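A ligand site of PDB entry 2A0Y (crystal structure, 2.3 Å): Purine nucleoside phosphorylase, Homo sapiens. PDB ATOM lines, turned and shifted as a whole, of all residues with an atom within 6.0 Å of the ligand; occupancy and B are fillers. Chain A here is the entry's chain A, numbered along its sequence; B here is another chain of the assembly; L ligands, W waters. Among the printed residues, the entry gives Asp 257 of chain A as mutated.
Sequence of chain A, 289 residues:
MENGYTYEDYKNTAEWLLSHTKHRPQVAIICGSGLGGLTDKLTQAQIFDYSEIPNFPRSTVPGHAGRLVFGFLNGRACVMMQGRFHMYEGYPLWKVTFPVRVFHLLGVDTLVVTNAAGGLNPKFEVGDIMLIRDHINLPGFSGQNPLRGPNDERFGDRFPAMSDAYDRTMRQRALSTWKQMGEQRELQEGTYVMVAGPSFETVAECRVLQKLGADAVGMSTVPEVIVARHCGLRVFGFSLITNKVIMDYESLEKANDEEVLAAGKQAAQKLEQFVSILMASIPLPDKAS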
ATOM      1  N   SER A  33     -12.595 -25.067  37.738  1.00  0.00           N
ATOM      2  CA  SER A  33     -12.777 -23.653  38.079  1.00  0.00           C
ATOM      3  C   SER A  33     -13.946 -23.422  39.034  1.00  0.00           C
ATOM      4  O   SER A  33     -15.077 -23.843  38.776  1.00  0.00           O
ATOM      5  CB  SER A  33     -12.989 -22.832  36.810  1.00  0.00           C
ATOM      6  OG  SER A  33     -13.287 -21.481  37.113  1.00  0.00           O
ATOM      7  N   HIS A  86      -3.176 -25.730  32.803  1.00  0.00           N
ATOM      8  CA  HIS A  86      -3.804 -25.666  31.491  1.00  0.00           C
ATOM      9  C   HIS A  86      -2.765 -25.465  30.414  1.00  0.00           C
ATOM     10  O   HIS A  86      -1.714 -24.857  30.637  1.00  0.00           O
ATOM     11  CB  HIS A  86      -4.801 -24.519  31.409  1.00  0.00           C
ATOM     12  CG  HIS A  86      -5.858 -24.544  32.461  1.00  0.00           C
ATOM     13  ND1 HIS A  86      -5.665 -24.025  33.717  1.00  0.00           N
ATOM     14  CD2 HIS A  86      -7.133 -25.006  32.437  1.00  0.00           C
ATOM     15  CE1 HIS A  86      -6.775 -24.158  34.429  1.00  0.00           C
ATOM     16  NE2 HIS A  86      -7.685 -24.746  33.662  1.00  0.00           N
ATOM     17  N   TYR A  88      -3.096 -23.606  27.761  1.00  0.00           N
ATOM     18  CA  TYR A  88      -3.026 -22.191  27.413  1.00  0.00           C
ATOM     19  C   TYR A  88      -2.044 -21.383  28.272  1.00  0.00           C
ATOM     20  O   TYR A  88      -1.631 -20.300  27.858  1.00  0.00           O
ATOM     21  CB  TYR A  88      -4.427 -21.537  27.439  1.00  0.00           C
ATOM     22  CG  TYR A  88      -5.132 -21.501  28.797  1.00  0.00           C
ATOM     23  CD1 TYR A  88      -4.647 -20.740  29.856  1.00  0.00           C
ATOM     24  CD2 TYR A  88      -6.298 -22.259  29.012  1.00  0.00           C
ATOM     25  CE1 TYR A  88      -5.277 -20.720  31.104  1.00  0.00           C
ATOM     26  CE2 TYR A  88      -6.947 -22.243  30.253  1.00  0.00           C
ATOM     27  CZ  TYR A  88      -6.431 -21.485  31.290  1.00  0.00           C
ATOM     28  OH  TYR A  88      -7.036 -21.516  32.520  1.00  0.00           O
ATOM     29  N   ALA A 116     -15.491 -26.316  34.528  1.00  0.00           N
ATOM     30  CA  ALA A 116     -16.551 -25.389  34.152  1.00  0.00           C
ATOM     31  C   ALA A 116     -16.533 -25.473  32.634  1.00  0.00           C
ATOM     32  O   ALA A 116     -15.501 -25.774  32.053  1.00  0.00           O
ATOM     33  CB  ALA A 116     -16.211 -23.983  34.600  1.00  0.00           C
ATOM     34  N   ALA A 117     -17.662 -25.204  31.986  1.00  0.00           N
ATOM     35  CA  ALA A 117     -17.703 -25.275  30.536  1.00  0.00           C
ATOM     36  C   ALA A 117     -18.874 -24.517  29.975  1.00  0.00           C
ATOM     37  O   ALA A 117     -19.911 -24.411  30.623  1.00  0.00           O
ATOM     38  CB  ALA A 117     -17.754 -26.720  30.080  1.00  0.00           C
ATOM     39  N   GLY A 118     -18.688 -23.995  28.773  1.00  0.00           N
ATOM     40  CA  GLY A 118     -19.747 -23.248  28.116  1.00  0.00           C
ATOM     41  C   GLY A 118     -20.716 -24.241  27.507  1.00  0.00           C
ATOM     42  O   GLY A 118     -20.309 -25.307  27.049  1.00  0.00           O
ATOM     43  N   GLY A 119     -21.997 -23.888  27.508  1.00  0.00           N
ATOM     44  CA  GLY A 119     -22.990 -24.785  26.953  1.00  0.00           C
ATOM     45  C   GLY A 119     -23.151 -24.620  25.467  1.00  0.00           C
ATOM     46  O   GLY A 119     -23.387 -23.516  24.967  1.00  0.00           O
ATOM     47  N   VAL A 195     -10.832 -27.328  23.624  1.00  0.00           N
ATOM     48  CA  VAL A 195     -10.169 -26.382  22.732  1.00  0.00           C
ATOM     49  C   VAL A 195      -9.104 -25.774  23.624  1.00  0.00           C
ATOM     50  O   VAL A 195      -9.283 -25.690  24.845  1.00  0.00           O
ATOM     51  CB  VAL A 195     -11.096 -25.250  22.227  1.00  0.00           C
ATOM     52  CG1 VAL A 195     -12.196 -25.817  21.357  1.00  0.00           C
ATOM     53  CG2 VAL A 195     -11.645 -24.444  23.393  1.00  0.00           C
ATOM     54  N   SER A 199      -8.461 -17.512  24.672  1.00  0.00           N
ATOM     55  CA  SER A 199      -9.546 -16.611  24.289  1.00  0.00           C
ATOM     56  C   SER A 199     -10.819 -17.434  24.056  1.00  0.00           C
ATOM     57  O   SER A 199     -10.741 -18.626  23.788  1.00  0.00           O
ATOM     58  CB  SER A 199      -9.174 -15.799  23.041  1.00  0.00           C
ATOM     59  OG  SER A 199      -8.868 -16.631  21.934  1.00  0.00           O
ATOM     60  N   PHE A 200     -11.982 -16.793  24.203  1.00  0.00           N
ATOM     61  CA  PHE A 200     -13.273 -17.474  24.021  1.00  0.00           C
ATOM     62  C   PHE A 200     -13.648 -17.629  22.548  1.00  0.00           C
ATOM     63  O   PHE A 200     -13.205 -16.851  21.682  1.00  0.00           O
ATOM     64  CB  PHE A 200     -14.387 -16.716  24.747  1.00  0.00           C
ATOM     65  CG  PHE A 200     -14.350 -16.874  26.247  1.00  0.00           C
ATOM     66  CD1 PHE A 200     -14.541 -18.128  26.830  1.00  0.00           C
ATOM     67  CD2 PHE A 200     -14.109 -15.780  27.069  1.00  0.00           C
ATOM     68  CE1 PHE A 200     -14.492 -18.293  28.211  1.00  0.00           C
ATOM     69  CE2 PHE A 200     -14.057 -15.924  28.463  1.00  0.00           C
ATOM     70  CZ  PHE A 200     -14.244 -17.184  29.039  1.00  0.00           C
ATOM     71  N   GLU A 201     -14.478 -18.626  22.266  1.00  0.00           N
ATOM     72  CA  GLU A 201     -14.907 -18.915  20.912  1.00  0.00           C
ATOM     73  C   GLU A 201     -15.758 -17.817  20.271  1.00  0.00           C
ATOM     74  O   GLU A 201     -16.436 -17.060  20.955  1.00  0.00           O
ATOM     75  CB  GLU A 201     -15.715 -20.220  20.876  1.00  0.00           C
ATOM     76  CG  GLU A 201     -15.024 -21.448  21.479  1.00  0.00           C
ATOM     77  CD  GLU A 201     -14.857 -21.360  22.990  1.00  0.00           C
ATOM     78  OE1 GLU A 201     -15.732 -20.800  23.677  1.00  0.00           O
ATOM     79  OE2 GLU A 201     -13.834 -21.886  23.504  1.00  0.00           O
ATOM     80  N   VAL A 217     -18.061 -27.047  26.162  1.00  0.00           N
ATOM     81  CA  VAL A 217     -16.701 -26.720  25.747  1.00  0.00           C
ATOM     82  C   VAL A 217     -15.834 -26.154  26.846  1.00  0.00           C
ATOM     83  O   VAL A 217     -16.254 -25.271  27.592  1.00  0.00           O
ATOM     84  CB  VAL A 217     -16.723 -25.706  24.579  1.00  0.00           C
ATOM     85  CG1 VAL A 217     -17.357 -24.401  25.028  1.00  0.00           C
ATOM     86  CG2 VAL A 217     -15.306 -25.476  24.076  1.00  0.00           C
ATOM     87  N   GLY A 218     -14.617 -26.677  26.944  1.00  0.00           N
ATOM     88  CA  GLY A 218     -13.667 -26.224  27.951  1.00  0.00           C
ATOM     89  C   GLY A 218     -12.245 -26.230  27.416  1.00  0.00           C
ATOM     90  O   GLY A 218     -12.005 -26.512  26.229  1.00  0.00           O
ATOM     91  N   MET A 219     -11.285 -25.927  28.284  1.00  0.00           N
ATOM     92  CA  MET A 219      -9.896 -25.864  27.869  1.00  0.00           C
ATOM     93  C   MET A 219      -9.021 -26.801  28.671  1.00  0.00           C
ATOM     94  O   MET A 219      -7.813 -26.576  28.800  1.00  0.00           O
ATOM     95  CB  MET A 219      -9.399 -24.434  28.024  1.00  0.00           C
ATOM     96  CG  MET A 219     -10.305 -23.429  27.342  1.00  0.00           C
ATOM     97  SD  MET A 219      -9.792 -21.733  27.635  1.00  0.00           S
ATOM     98  CE  MET A 219     -11.074 -20.848  26.794  1.00  0.00           C
ATOM     99  N   THR A 242     -21.401 -23.021  33.116  1.00  0.00           N
ATOM    100  CA  THR A 242     -21.356 -21.708  33.736  1.00  0.00           C
ATOM    101  C   THR A 242     -21.863 -20.611  32.803  1.00  0.00           C
ATOM    102  O   THR A 242     -22.007 -19.465  33.214  1.00  0.00           O
ATOM    103  CB  THR A 242     -19.937 -21.346  34.143  1.00  0.00           C
ATOM    104  OG1 THR A 242     -19.115 -21.282  32.954  1.00  0.00           O
ATOM    105  CG2 THR A 242     -19.364 -22.382  35.105  1.00  0.00           C
ATOM    106  N   ASN A 243     -22.128 -20.964  31.555  1.00  0.00           N
ATOM    107  CA  ASN A 243     -22.589 -19.970  30.598  1.00  0.00           C
ATOM    108  C   ASN A 243     -22.981 -20.650  29.306  1.00  0.00           C
ATOM    109  O   ASN A 243     -22.534 -21.752  29.020  1.00  0.00           O
ATOM    110  CB  ASN A 243     -21.455 -18.980  30.314  1.00  0.00           C
ATOM    111  CG  ASN A 243     -20.186 -19.669  29.808  1.00  0.00           C
ATOM    112  OD1 ASN A 243     -19.570 -20.463  30.522  1.00  0.00           O
ATOM    113  ND2 ASN A 243     -19.810 -19.378  28.567  1.00  0.00           N
ATOM    114  N   VAL A 245     -22.715 -20.433  25.416  1.00  0.00           N
ATOM    115  CA  VAL A 245     -21.920 -19.793  24.380  1.00  0.00           C
ATOM    116  C   VAL A 245     -22.786 -19.081  23.359  1.00  0.00           C
ATOM    117  O   VAL A 245     -23.818 -19.598  22.927  1.00  0.00           O
ATOM    118  CB  VAL A 245     -21.019 -20.820  23.673  1.00  0.00           C
ATOM    119  CG1 VAL A 245     -20.072 -21.445  24.673  1.00  0.00           C
ATOM    120  CG2 VAL A 245     -21.853 -21.888  23.021  1.00  0.00           C
ATOM    121  N   ALA A 255     -19.013 -13.864  26.640  1.00  0.00           N
ATOM    122  CA  ALA A 255     -18.505 -14.771  27.665  1.00  0.00           C
ATOM    123  C   ALA A 255     -17.384 -14.054  28.418  1.00  0.00           C
ATOM    124  O   ALA A 255     -16.570 -13.365  27.812  1.00  0.00           O
ATOM    125  CB  ALA A 255     -17.975 -16.050  27.020  1.00  0.00           C
ATOM    126  N   ASN A 256     -17.352 -14.226  29.730  1.00  0.00           N
ATOM    127  CA  ASN A 256     -16.330 -13.579  30.548  1.00  0.00           C
ATOM    128  C   ASN A 256     -16.028 -14.393  31.803  1.00  0.00           C
ATOM    129  O   ASN A 256     -16.898 -15.081  32.330  1.00  0.00           O
ATOM    130  CB  ASN A 256     -16.790 -12.163  30.913  1.00  0.00           C
ATOM    131  CG  ASN A 256     -18.165 -12.143  31.551  1.00  0.00           C
ATOM    132  OD1 ASN A 256     -18.341 -12.510  32.718  1.00  0.00           O
ATOM    133  ND2 ASN A 256     -19.165 -11.723  30.782  1.00  0.00           N
ATOM    134  N   ASP A 257     -14.792 -14.300  32.268  1.00  0.00           N
ATOM    135  CA  ASP A 257     -14.364 -15.052  33.449  1.00  0.00           C
ATOM    136  C   ASP A 257     -15.125 -14.662  34.721  1.00  0.00           C
ATOM    137  O   ASP A 257     -15.098 -15.390  35.722  1.00  0.00           O
ATOM    138  CB  ASP A 257     -12.858 -14.858  33.661  1.00  0.00           C
ATOM    139  CG  ASP A 257     -12.305 -15.782  34.719  1.00  0.00           C
ATOM    140  OD1 ASP A 257     -12.400 -17.017  34.529  1.00  0.00           O
ATOM    141  OD2 ASP A 257     -11.759 -15.277  35.721  1.00  0.00           O
ATOM    142  N   GLU A 258     -15.805 -13.520  34.688  1.00  0.00           N
ATOM    143  CA  GLU A 258     -16.577 -13.069  35.848  1.00  0.00           C
ATOM    144  C   GLU A 258     -17.800 -13.954  36.006  1.00  0.00           C
ATOM    145  O   GLU A 258     -18.058 -14.479  37.085  1.00  0.00           O
ATOM    146  CB  GLU A 258     -17.005 -11.605  35.662  1.00  0.00           C
ATOM    147  CG  GLU A 258     -15.847 -10.661  35.421  1.00  0.00           C
ATOM    148  CD  GLU A 258     -14.829 -10.712  36.543  1.00  0.00           C
ATOM    149  OE1 GLU A 258     -15.118 -10.175  37.639  1.00  0.00           O
ATOM    150  OE2 GLU A 258     -13.735 -11.297  36.327  1.00  0.00           O
ATOM    151  N   VAL A 260     -18.326 -16.921  34.664  1.00  0.00           N
ATOM    152  CA  VAL A 260     -17.870 -18.283  34.936  1.00  0.00           C
ATOM    153  C   VAL A 260     -17.610 -18.529  36.420  1.00  0.00           C
ATOM    154  O   VAL A 260     -18.042 -19.545  36.974  1.00  0.00           O
ATOM    155  CB  VAL A 260     -16.591 -18.635  34.142  1.00  0.00           C
ATOM    156  CG1 VAL A 260     -16.123 -20.036  34.485  1.00  0.00           C
ATOM    157  CG2 VAL A 260     -16.864 -18.509  32.655  1.00  0.00           C
ATOM    158  N   LEU A 261     -16.887 -17.616  37.059  1.00  0.00           N
ATOM    159  CA  LEU A 261     -16.577 -17.752  38.479  1.00  0.00           C
ATOM    160  C   LEU A 261     -17.828 -17.491  39.323  1.00  0.00           C
ATOM    161  O   LEU A 261     -18.029 -18.134  40.354  1.00  0.00           O
ATOM    162  CB  LEU A 261     -15.477 -16.761  38.879  1.00  0.00           C
ATOM    163  CG  LEU A 261     -14.089 -17.011  38.274  1.00  0.00           C
ATOM    164  CD1 LEU A 261     -13.172 -15.841  38.595  1.00  0.00           C
ATOM    165  CD2 LEU A 261     -13.513 -18.320  38.812  1.00  0.00           C
ATOM    166  N   PHE B 159      -8.668 -14.203  29.680  1.00  0.00           N
ATOM    167  CA  PHE B 159      -9.625 -14.842  28.770  1.00  0.00           C
ATOM    168  C   PHE B 159     -10.445 -13.845  27.940  1.00  0.00           C
ATOM    169  O   PHE B 159     -11.644 -13.693  28.156  1.00  0.00           O
ATOM    170  CB  PHE B 159     -10.591 -15.723  29.578  1.00  0.00           C
ATOM    171  CG  PHE B 159      -9.911 -16.650  30.555  1.00  0.00           C
ATOM    172  CD1 PHE B 159      -9.234 -17.772  30.119  1.00  0.00           C
ATOM    173  CD2 PHE B 159      -9.946 -16.376  31.922  1.00  0.00           C
ATOM    174  CE1 PHE B 159      -8.605 -18.641  31.032  1.00  0.00           C
ATOM    175  CE2 PHE B 159      -9.323 -17.226  32.846  1.00  0.00           C
ATOM    176  CZ  PHE B 159      -8.640 -18.367  32.399  1.00  0.00           C
HETATM  177  O1  LIG L   1     -13.317 -18.382  32.756  1.00  0.00           O
HETATM  178  C1  LIG L   1     -12.380 -19.213  32.101  1.00  0.00           C
HETATM  179  C2  LIG L   1     -11.933 -20.574  32.485  1.00  0.00           C
HETATM  180  C3  LIG L   1     -13.101 -21.482  32.503  1.00  0.00           C
HETATM  181  C4  LIG L   1     -10.931 -21.152  31.545  1.00  0.00           C
HETATM  182  O2  LIG L   1      -9.803 -21.812  32.122  1.00  0.00           O
HETATM  183  C5  LIG L   1     -11.902 -21.912  30.724  1.00  0.00           C
HETATM  184  N1  LIG L   1     -12.811 -22.589  31.615  1.00  0.00           N
HETATM  185  C6  LIG L   1     -14.018 -23.124  31.022  1.00  0.00           C
HETATM  186  C7  LIG L   1     -15.062 -22.405  30.250  1.00  0.00           C
HETATM  187  C8  LIG L   1     -16.222 -21.800  30.695  1.00  0.00           C
HETATM  188  N2  LIG L   1     -16.938 -21.233  29.764  1.00  0.00           N
HETATM  189  C9  LIG L   1     -16.240 -21.448  28.590  1.00  0.00           C
HETATM  190  C10 LIG L   1     -16.546 -21.032  27.216  1.00  0.00           C
HETATM  191  O3  LIG L   1     -17.519 -20.395  26.844  1.00  0.00           O
HETATM  192  N3  LIG L   1     -15.572 -21.443  26.254  1.00  0.00           N
HETATM  193  C11 LIG L   1     -14.400 -22.190  26.573  1.00  0.00           C
HETATM  194  N4  LIG L   1     -14.113 -22.574  27.865  1.00  0.00           N
HETATM  195  C12 LIG L   1     -15.070 -22.176  28.845  1.00  0.00           C
HETATM  196  O   HOH W   1     -10.745 -24.662  31.076  1.00  0.00           O
HETATM  197  O   HOH W   2     -17.631 -18.837  24.602  1.00  0.00           O
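An oxygen (O1) of the ligand lies within hydrogen-bond range of the side-chain carboxylate of Asp 257, 2.4 Å away. The side-chain carboxylate (OE1) of Glu 201 is in hydrogen-bond range of a nitrogen (N3) of the ligand. The side-chain hydroxyl (OH) of Tyr 88 is in hydrogen-bond range of an oxygen (O2) of the ligand (2.8 Å). OD1 of Asn 243 is in hydrogen-bond range of N2 of the ligand, at 2.8 Å. A nitrogen (N2) of the ligand sits close to the backbone NH (N) of Gly 118 (3.4 Å). N4 of the ligand sits close to O of Val 217.
A ring nitrogen (ND1) of His 86 lies within hydrogen-bond range of the side-chain hydroxyl (OH) of Tyr 88 (3.1 Å). OD1 of Asn 243 lies within hydrogen-bond range of OG1 of Thr 242 (2.6 Å). O of Asn 243 is in hydrogen-bond range of N of Gly 119 (2.7 Å). O of Gly 118 lies within hydrogen-bond range of N of Val 217 (3.0 Å). The backbone NH (N) of Val 245 sits close to the backbone carbonyl oxygen (O) of Gly 119. O of Gly 218 sits at hydrogen-bond distance from N of Val 195 (3.0 Å). O of Ala 117 lies within hydrogen-bond range of N of Thr 242 (3.2 Å).
NE2 of His 86 touches O2 of the ligand, at 3.9 Å. Ala 116 touches the ligand. Ala 117 touches the ligand (CA to C8, 3.8 Å). Phe 200 touches the ligand (CD1 to N3, 3.5 Å). Gly 218 touches the ligand. Met 219 touches the ligand. Thr 242 touches the ligand (OG1 to C8, 3.7 Å). Val 245 touches the ligand. CG2 of Val 260 touches O1 of the ligand, 3.6 Å away. Phe 159 of chain B touches the ligand (CE1 to C4, 3.5 Å). Hydrophobic or aromatic side chains that line the ligand: Tyr 88, Phe 200, Val 217, Met 219, Val 245, Val 260 and Phe 159 of chain B. 16 residues have an atom within 4 Å of the ligand: His 86, Tyr 88, Ala 116, Ala 117, Gly 118, Phe 200, Glu 201, Val 217, Gly 218, Met 219, Thr 242, Asn 243, Val 245, Asp 257, Val 260 and Phe 159 of chain B. The nearest printed residue that does not touch the ligand is Ala 255 (4.4 Å).
Water W2 lies within hydrogen-bond range of an oxygen (O3) of the ligand (2.7 Å) and the side-chain carboxylate of Glu 201 (2.9 Å). Water W1 lies within hydrogen-bond range of a nitrogen (N1) of the ligand (3.0 Å) and the backbone NH of Met 219 (3.1 Å).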
